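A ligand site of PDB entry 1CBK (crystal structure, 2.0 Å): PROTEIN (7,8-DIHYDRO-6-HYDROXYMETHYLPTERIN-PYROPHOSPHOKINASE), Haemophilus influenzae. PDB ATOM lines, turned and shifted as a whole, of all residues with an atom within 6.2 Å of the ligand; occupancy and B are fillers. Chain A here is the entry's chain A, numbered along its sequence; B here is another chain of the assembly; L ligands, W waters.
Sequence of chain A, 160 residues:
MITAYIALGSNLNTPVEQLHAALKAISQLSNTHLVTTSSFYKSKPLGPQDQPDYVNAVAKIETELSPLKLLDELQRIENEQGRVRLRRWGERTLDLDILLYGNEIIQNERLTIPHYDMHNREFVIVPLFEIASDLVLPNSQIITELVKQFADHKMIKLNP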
ATOM      1  N   LEU A   8      13.232  -7.710  21.642  1.00  0.00           N
ATOM      2  CA  LEU A   8      13.857  -7.734  22.962  1.00  0.00           C
ATOM      3  C   LEU A   8      14.627  -6.445  23.205  1.00  0.00           C
ATOM      4  O   LEU A   8      15.327  -5.966  22.325  1.00  0.00           O
ATOM      5  CB  LEU A   8      14.841  -8.923  23.105  1.00  0.00           C
ATOM      6  CG  LEU A   8      14.433 -10.366  22.805  1.00  0.00           C
ATOM      7  CD1 LEU A   8      14.573 -10.660  21.307  1.00  0.00           C
ATOM      8  CD2 LEU A   8      15.296 -11.301  23.636  1.00  0.00           C
ATOM      9  N   GLY A   9      14.545  -5.921  24.424  1.00  0.00           N
ATOM     10  CA  GLY A   9      15.281  -4.698  24.748  1.00  0.00           C
ATOM     11  C   GLY A   9      15.653  -4.658  26.207  1.00  0.00           C
ATOM     12  O   GLY A   9      14.976  -5.281  27.032  1.00  0.00           O
ATOM     13  N   SER A  10      16.750  -3.985  26.539  1.00  0.00           N
ATOM     14  CA  SER A  10      17.190  -3.879  27.946  1.00  0.00           C
ATOM     15  C   SER A  10      18.197  -2.773  28.078  1.00  0.00           C
ATOM     16  O   SER A  10      18.973  -2.537  27.144  1.00  0.00           O
ATOM     17  CB  SER A  10      17.867  -5.181  28.415  1.00  0.00           C
ATOM     18  OG  SER A  10      18.557  -5.032  29.667  1.00  0.00           O
ATOM     19  N   SER A  43      21.317   1.278  21.102  1.00  0.00           N
ATOM     20  CA  SER A  43      20.565   2.400  20.582  1.00  0.00           C
ATOM     21  C   SER A  43      20.285   3.478  21.624  1.00  0.00           C
ATOM     22  O   SER A  43      20.186   3.186  22.816  1.00  0.00           O
ATOM     23  CB  SER A  43      19.230   1.880  20.029  1.00  0.00           C
ATOM     24  OG  SER A  43      18.495   1.215  21.058  1.00  0.00           O
ATOM     25  N   LYS A  44      20.118   4.710  21.158  1.00  0.00           N
ATOM     26  CA  LYS A  44      19.805   5.857  22.004  1.00  0.00           C
ATOM     27  C   LYS A  44      18.438   5.612  22.598  1.00  0.00           C
ATOM     28  O   LYS A  44      17.541   5.119  21.898  1.00  0.00           O
ATOM     29  CB  LYS A  44      19.779   7.097  21.108  1.00  0.00           C
ATOM     30  CG  LYS A  44      19.478   8.402  21.828  1.00  0.00           C
ATOM     31  CD  LYS A  44      19.392   9.570  20.855  1.00  0.00           C
ATOM     32  CE  LYS A  44      19.660  10.888  21.566  1.00  0.00           C
ATOM     33  NZ  LYS A  44      19.431  12.081  20.701  1.00  0.00           N
ATOM     34  N   PRO A  45      18.244   5.937  23.874  1.00  0.00           N
ATOM     35  CA  PRO A  45      16.934   5.732  24.492  1.00  0.00           C
ATOM     36  C   PRO A  45      15.788   6.517  23.853  1.00  0.00           C
ATOM     37  O   PRO A  45      15.979   7.652  23.407  1.00  0.00           O
ATOM     38  CB  PRO A  45      17.143   6.248  25.920  1.00  0.00           C
ATOM     39  CG  PRO A  45      18.578   6.068  26.144  1.00  0.00           C
ATOM     40  CD  PRO A  45      19.192   6.483  24.851  1.00  0.00           C
ATOM     41  N   LEU A  46      14.632   5.875  23.731  1.00  0.00           N
ATOM     42  CA  LEU A  46      13.429   6.537  23.254  1.00  0.00           C
ATOM     43  C   LEU A  46      12.748   6.857  24.604  1.00  0.00           C
ATOM     44  O   LEU A  46      12.297   5.958  25.315  1.00  0.00           O
ATOM     45  CB  LEU A  46      12.533   5.584  22.421  1.00  0.00           C
ATOM     46  CG  LEU A  46      11.125   6.138  22.119  1.00  0.00           C
ATOM     47  CD1 LEU A  46      11.243   7.475  21.296  1.00  0.00           C
ATOM     48  CD2 LEU A  46      10.304   5.095  21.370  1.00  0.00           C
ATOM     49  N   GLY A  47      12.721   8.137  24.983  1.00  0.00           N
ATOM     50  CA  GLY A  47      12.134   8.526  26.248  1.00  0.00           C
ATOM     51  C   GLY A  47      13.081   9.474  26.945  1.00  0.00           C
ATOM     52  O   GLY A  47      13.841  10.174  26.265  1.00  0.00           O
ATOM     53  N   PRO A  48      13.011   9.594  28.285  1.00  0.00           N
ATOM     54  CA  PRO A  48      13.910  10.480  29.044  1.00  0.00           C
ATOM     55  C   PRO A  48      15.341  10.125  28.599  1.00  0.00           C
ATOM     56  O   PRO A  48      15.662   8.951  28.384  1.00  0.00           O
ATOM     57  CB  PRO A  48      13.693  10.030  30.489  1.00  0.00           C
ATOM     58  CG  PRO A  48      12.301   9.516  30.504  1.00  0.00           C
ATOM     59  CD  PRO A  48      12.059   8.894  29.165  1.00  0.00           C
ATOM     60  N   GLN A  51      19.082   8.060  30.915  1.00  0.00           N
ATOM     61  CA  GLN A  51      19.055   6.623  31.196  1.00  0.00           C
ATOM     62  C   GLN A  51      20.084   5.998  30.279  1.00  0.00           C
ATOM     63  O   GLN A  51      20.499   6.630  29.287  1.00  0.00           O
ATOM     64  CB  GLN A  51      17.660   6.016  30.972  1.00  0.00           C
ATOM     65  CG  GLN A  51      17.175   6.038  29.553  1.00  0.00           C
ATOM     66  CD  GLN A  51      15.778   5.443  29.429  1.00  0.00           C
ATOM     67  OE1 GLN A  51      15.521   4.340  29.901  1.00  0.00           O
ATOM     68  NE2 GLN A  51      14.862   6.202  28.844  1.00  0.00           N
ATOM     69  N   ASP A  53      21.884   3.745  27.341  1.00  0.00           N
ATOM     70  CA  ASP A  53      21.509   3.329  25.995  1.00  0.00           C
ATOM     71  C   ASP A  53      20.997   1.896  26.107  1.00  0.00           C
ATOM     72  O   ASP A  53      21.483   1.115  26.955  1.00  0.00           O
ATOM     73  CB  ASP A  53      22.714   3.339  25.075  1.00  0.00           C
ATOM     74  CG  ASP A  53      23.101   4.736  24.596  1.00  0.00           C
ATOM     75  OD1 ASP A  53      22.365   5.703  24.874  1.00  0.00           O
ATOM     76  OD2 ASP A  53      24.143   4.830  23.922  1.00  0.00           O
ATOM     77  N   TYR A  54      20.098   1.515  25.216  1.00  0.00           N
ATOM     78  CA  TYR A  54      19.530   0.178  25.217  1.00  0.00           C
ATOM     79  C   TYR A  54      20.263  -0.769  24.320  1.00  0.00           C
ATOM     80  O   TYR A  54      21.024  -0.326  23.443  1.00  0.00           O
ATOM     81  CB  TYR A  54      18.088   0.226  24.719  1.00  0.00           C
ATOM     82  CG  TYR A  54      17.098   0.714  25.745  1.00  0.00           C
ATOM     83  CD1 TYR A  54      16.998   2.071  26.080  1.00  0.00           C
ATOM     84  CD2 TYR A  54      16.263  -0.196  26.381  1.00  0.00           C
ATOM     85  CE1 TYR A  54      16.059   2.497  27.047  1.00  0.00           C
ATOM     86  CE2 TYR A  54      15.328   0.218  27.336  1.00  0.00           C
ATOM     87  CZ  TYR A  54      15.232   1.553  27.662  1.00  0.00           C
ATOM     88  OH  TYR A  54      14.304   1.913  28.600  1.00  0.00           O
ATOM     89  N   VAL A  55      20.096  -2.067  24.576  1.00  0.00           N
ATOM     90  CA  VAL A  55      20.650  -3.114  23.696  1.00  0.00           C
ATOM     91  C   VAL A  55      19.344  -3.787  23.186  1.00  0.00           C
ATOM     92  O   VAL A  55      18.463  -4.148  24.002  1.00  0.00           O
ATOM     93  CB  VAL A  55      21.604  -4.111  24.402  1.00  0.00           C
ATOM     94  CG1 VAL A  55      22.093  -5.169  23.394  1.00  0.00           C
ATOM     95  CG2 VAL A  55      22.818  -3.365  24.946  1.00  0.00           C
ATOM     96  N   ASN A  56      19.202  -3.834  21.865  1.00  0.00           N
ATOM     97  CA  ASN A  56      18.014  -4.368  21.209  1.00  0.00           C
ATOM     98  C   ASN A  56      18.277  -5.471  20.200  1.00  0.00           C
ATOM     99  O   ASN A  56      19.324  -5.537  19.589  1.00  0.00           O
ATOM    100  CB  ASN A  56      17.283  -3.233  20.457  1.00  0.00           C
ATOM    101  CG  ASN A  56      16.559  -2.279  21.384  1.00  0.00           C
ATOM    102  OD1 ASN A  56      17.005  -1.159  21.603  1.00  0.00           O
ATOM    103  ND2 ASN A  56      15.425  -2.711  21.898  1.00  0.00           N
ATOM    104  N   ARG A  88       8.186   4.868  34.197  1.00  0.00           N
ATOM    105  CA  ARG A  88       7.585   4.767  32.855  1.00  0.00           C
ATOM    106  C   ARG A  88       8.547   5.455  31.870  1.00  0.00           C
ATOM    107  O   ARG A  88       9.148   6.479  32.166  1.00  0.00           O
ATOM    108  CB  ARG A  88       6.216   5.442  32.770  1.00  0.00           C
ATOM    109  CG  ARG A  88       5.532   5.133  31.441  1.00  0.00           C
ATOM    110  CD  ARG A  88       4.281   5.948  31.209  1.00  0.00           C
ATOM    111  NE  ARG A  88       3.171   5.555  32.086  1.00  0.00           N
ATOM    112  CZ  ARG A  88       2.005   6.184  32.156  1.00  0.00           C
ATOM    113  NH1 ARG A  88       1.761   7.285  31.440  1.00  0.00           N
ATOM    114  NH2 ARG A  88       1.068   5.728  32.974  1.00  0.00           N
ATOM    115  N   TRP A  89       8.703   4.833  30.699  1.00  0.00           N
ATOM    116  CA  TRP A  89       9.619   5.281  29.659  1.00  0.00           C
ATOM    117  C   TRP A  89      11.072   5.239  30.085  1.00  0.00           C
ATOM    118  O   TRP A  89      11.945   5.671  29.319  1.00  0.00           O
ATOM    119  CB  TRP A  89       9.298   6.698  29.143  1.00  0.00           C
ATOM    120  CG  TRP A  89       7.939   6.871  28.627  1.00  0.00           C
ATOM    121  CD1 TRP A  89       6.921   7.550  29.220  1.00  0.00           C
ATOM    122  CD2 TRP A  89       7.431   6.405  27.377  1.00  0.00           C
ATOM    123  NE1 TRP A  89       5.807   7.551  28.410  1.00  0.00           N
ATOM    124  CE2 TRP A  89       6.097   6.841  27.266  1.00  0.00           C
ATOM    125  CE3 TRP A  89       7.975   5.659  26.323  1.00  0.00           C
ATOM    126  CZ2 TRP A  89       5.296   6.571  26.150  1.00  0.00           C
ATOM    127  CZ3 TRP A  89       7.169   5.387  25.199  1.00  0.00           C
ATOM    128  CH2 TRP A  89       5.854   5.843  25.132  1.00  0.00           C
ATOM    129  N   GLY A  90      11.345   4.690  31.265  1.00  0.00           N
ATOM    130  CA  GLY A  90      12.713   4.633  31.744  1.00  0.00           C
ATOM    131  C   GLY A  90      13.356   3.251  31.754  1.00  0.00           C
ATOM    132  O   GLY A  90      12.919   2.334  31.049  1.00  0.00           O
ATOM    133  N   ARG A  92      14.769  -0.499  32.395  1.00  0.00           N
ATOM    134  CA  ARG A  92      14.154  -1.818  32.590  1.00  0.00           C
ATOM    135  C   ARG A  92      15.227  -2.863  32.279  1.00  0.00           C
ATOM    136  O   ARG A  92      16.017  -2.698  31.340  1.00  0.00           O
ATOM    137  CB  ARG A  92      12.975  -1.998  31.621  1.00  0.00           C
ATOM    138  CG  ARG A  92      13.417  -1.950  30.145  1.00  0.00           C
ATOM    139  CD  ARG A  92      12.355  -1.389  29.252  1.00  0.00           C
ATOM    140  NE  ARG A  92      11.949  -0.081  29.732  1.00  0.00           N
ATOM    141  CZ  ARG A  92      10.684   0.251  29.926  1.00  0.00           C
ATOM    142  NH1 ARG A  92       9.707  -0.612  29.632  1.00  0.00           N
ATOM    143  NH2 ARG A  92      10.376   1.468  30.384  1.00  0.00           N
ATOM    144  N   ASP A  95      12.500  -6.394  28.336  1.00  0.00           N
ATOM    145  CA  ASP A  95      11.158  -6.294  27.764  1.00  0.00           C
ATOM    146  C   ASP A  95      11.143  -7.270  26.569  1.00  0.00           C
ATOM    147  O   ASP A  95      12.055  -7.226  25.750  1.00  0.00           O
ATOM    148  CB  ASP A  95      10.848  -4.881  27.229  1.00  0.00           C
ATOM    149  CG  ASP A  95      10.015  -4.059  28.193  1.00  0.00           C
ATOM    150  OD1 ASP A  95       9.664  -4.545  29.277  1.00  0.00           O
ATOM    151  OD2 ASP A  95       9.698  -2.902  27.855  1.00  0.00           O
ATOM    152  N   ARG A 121       9.968   2.504  15.197  1.00  0.00           N
ATOM    153  CA  ARG A 121      11.141   2.413  16.051  1.00  0.00           C
ATOM    154  C   ARG A 121      12.319   1.824  15.307  1.00  0.00           C
ATOM    155  O   ARG A 121      12.264   0.679  14.864  1.00  0.00           O
ATOM    156  CB  ARG A 121      10.824   1.562  17.282  1.00  0.00           C
ATOM    157  CG  ARG A 121       9.863   2.240  18.237  1.00  0.00           C
ATOM    158  CD  ARG A 121       9.502   1.343  19.411  1.00  0.00           C
ATOM    159  NE  ARG A 121       8.535   1.985  20.292  1.00  0.00           N
ATOM    160  CZ  ARG A 121       8.254   1.586  21.517  1.00  0.00           C
ATOM    161  NH1 ARG A 121       8.882   0.549  22.041  1.00  0.00           N
ATOM    162  NH2 ARG A 121       7.342   2.236  22.231  1.00  0.00           N
ATOM    163  N   GLU A 122      13.417   2.572  15.229  1.00  0.00           N
ATOM    164  CA  GLU A 122      14.609   2.110  14.542  1.00  0.00           C
ATOM    165  C   GLU A 122      15.181   0.815  15.123  1.00  0.00           C
ATOM    166  O   GLU A 122      15.734   0.001  14.370  1.00  0.00           O
ATOM    167  CB  GLU A 122      15.697   3.184  14.600  1.00  0.00           C
ATOM    168  CG  GLU A 122      16.191   3.511  16.023  1.00  0.00           C
ATOM    169  CD  GLU A 122      17.287   4.568  16.042  1.00  0.00           C
ATOM    170  OE1 GLU A 122      17.752   4.988  14.956  1.00  0.00           O
ATOM    171  OE2 GLU A 122      17.689   4.965  17.148  1.00  0.00           O
ATOM    172  N   PHE A 123      15.092   0.662  16.435  1.00  0.00           N
ATOM    173  CA  PHE A 123      15.649  -0.499  17.118  1.00  0.00           C
ATOM    174  C   PHE A 123      14.778  -1.742  17.023  1.00  0.00           C
ATOM    175  O   PHE A 123      15.062  -2.764  17.665  1.00  0.00           O
ATOM    176  CB  PHE A 123      15.978  -0.163  18.582  1.00  0.00           C
ATOM    177  CG  PHE A 123      14.885   0.541  19.311  1.00  0.00           C
ATOM    178  CD1 PHE A 123      13.894  -0.180  19.960  1.00  0.00           C
ATOM    179  CD2 PHE A 123      14.861   1.928  19.382  1.00  0.00           C
ATOM    180  CE1 PHE A 123      12.882   0.463  20.671  1.00  0.00           C
ATOM    181  CE2 PHE A 123      13.856   2.591  20.084  1.00  0.00           C
ATOM    182  CZ  PHE A 123      12.873   1.859  20.729  1.00  0.00           C
ATOM    183  N   TYR B 116       6.157   9.419  23.994  1.00  0.00           N
ATOM    184  CA  TYR B 116       7.295   9.267  23.102  1.00  0.00           C
ATOM    185  C   TYR B 116       7.057   8.614  21.756  1.00  0.00           C
ATOM    186  O   TYR B 116       7.803   8.877  20.811  1.00  0.00           O
ATOM    187  CB  TYR B 116       8.492   8.672  23.844  1.00  0.00           C
ATOM    188  CG  TYR B 116       9.012   9.631  24.908  1.00  0.00           C
ATOM    189  CD1 TYR B 116       8.466   9.638  26.193  1.00  0.00           C
ATOM    190  CD2 TYR B 116       9.983  10.579  24.604  1.00  0.00           C
ATOM    191  CE1 TYR B 116       8.865  10.598  27.154  1.00  0.00           C
ATOM    192  CE2 TYR B 116      10.399  11.537  25.554  1.00  0.00           C
ATOM    193  CZ  TYR B 116       9.836  11.529  26.817  1.00  0.00           C
ATOM    194  OH  TYR B 116      10.245  12.451  27.743  1.00  0.00           O
ATOM    195  N   ASP B 117       5.998   7.831  21.615  1.00  0.00           N
ATOM    196  CA  ASP B 117       5.773   7.215  20.299  1.00  0.00           C
ATOM    197  C   ASP B 117       5.306   8.273  19.303  1.00  0.00           C
ATOM    198  O   ASP B 117       5.601   8.187  18.105  1.00  0.00           O
ATOM    199  CB  ASP B 117       4.799   6.048  20.398  1.00  0.00           C
ATOM    200  CG  ASP B 117       5.457   4.813  20.989  1.00  0.00           C
ATOM    201  OD1 ASP B 117       6.564   4.457  20.537  1.00  0.00           O
ATOM    202  OD2 ASP B 117       4.865   4.213  21.899  1.00  0.00           O
HETATM  203  N1  LIG L   1      14.542   2.857  23.877  1.00  0.00           N
HETATM  204  C1  LIG L   1      15.359   2.015  23.156  1.00  0.00           C
HETATM  205  N2  LIG L   1      16.388   2.584  22.457  1.00  0.00           N
HETATM  206  N3  LIG L   1      15.196   0.672  23.108  1.00  0.00           N
HETATM  207  C2  LIG L   1      14.184   0.064  23.767  1.00  0.00           C
HETATM  208  O1  LIG L   1      14.047  -1.176  23.761  1.00  0.00           O
HETATM  209  C3  LIG L   1      13.261   0.871  24.498  1.00  0.00           C
HETATM  210  N4  LIG L   1      12.263   0.320  25.133  1.00  0.00           N
HETATM  211  C4  LIG L   1      11.328   1.033  25.859  1.00  0.00           C
HETATM  212  C5  LIG L   1      11.360   2.580  25.798  1.00  0.00           C
HETATM  213  C6  LIG L   1      10.292   3.123  24.776  1.00  0.00           C
HETATM  214  C7  LIG L   1      11.176   3.187  27.195  1.00  0.00           C
HETATM  215  N5  LIG L   1      12.649   3.106  25.250  1.00  0.00           N
HETATM  216  C8  LIG L   1      13.513   2.316  24.519  1.00  0.00           C
HETATM  217  O2  LIG L   1      10.506   0.325  26.522  1.00  0.00           O
HETATM  218  O   HOH W   1       7.947   1.418  27.008  1.00  0.00           O
HETATM  219  O   HOH W   2      12.102  -2.724  24.795  1.00  0.00           O
HETATM  220  O   HOH W   3       9.399  -2.115  25.171  1.00  0.00           O
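Merely in contact with the ligand: Gly 9 (3.9 Å), Pro 45 (3.8 Å), Tyr 54 (3.3 Å), Trp 89 (3.4 Å), Asp 95 (3.6 Å), Arg 121 (3.996 Å) and Phe 123 (3.4 Å).
Within 4 Å of the ligand: Gly 9, Ser 43, Lys 44, Pro 45, Leu 46, Tyr 54, Asn 56, Trp 89, Arg 92, Asp 95, Arg 121 and Phe 123.
The nearest printed residue that does not touch the ligand is Gly 90 (4.3 Å).
Water W3 bridges OD2 of Asp 95 and O2 of the ligand.
The backbone carbonyl oxygen of Leu 8 lies within hydrogen-bond range of the side-chain amide nitrogen of Asn 56, at 3.3 Å.
OG of Ser 43 sits at hydrogen-bond distance from OD1 of Asn 56, 2.9 Å away.
O of Trp 89 lies within hydrogen-bond range of NE2 of Gln 51.
The side-chain hydroxyl (OH) of Tyr 54 lies within hydrogen-bond range of the backbone carbonyl oxygen (O) of Gly 90, 2.8 Å away.
The backbone carbonyl oxygen (O) of Gly 9 is in hydrogen-bond range of the backbone NH (N) of Asp 95 (3.0 Å).
The backbone carbonyl oxygen (O) of Gly 90 is in hydrogen-bond range of the guanidinium group (NH2) of Arg 92.
The side-chain hydroxyl (OH) of Tyr 54 lies within hydrogen-bond range of the guanidinium group (NE) of Arg 92 (3.3 Å).
NH2 of Arg 121 is in salt-bridge range of OD1 of Asp 117 of chain B, 2.9 Å away.
O of Lys 44 sits at hydrogen-bond distance from N2 of the ligand (2.8 Å).
O of Leu 46 lies within hydrogen-bond range of N5 of the ligand.
NH1 of Arg 92 lies within hydrogen-bond range of O2 of the ligand (3.3 Å).
A nitrogen (N1) of the ligand is in hydrogen-bond range of the backbone NH of Leu 46.
ND2 of Asn 56 is in hydrogen-bond range of O1 of the ligand (2.8 Å).
N2 of the ligand lies within hydrogen-bond range of OG of Ser 43, 2.9 Å away.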
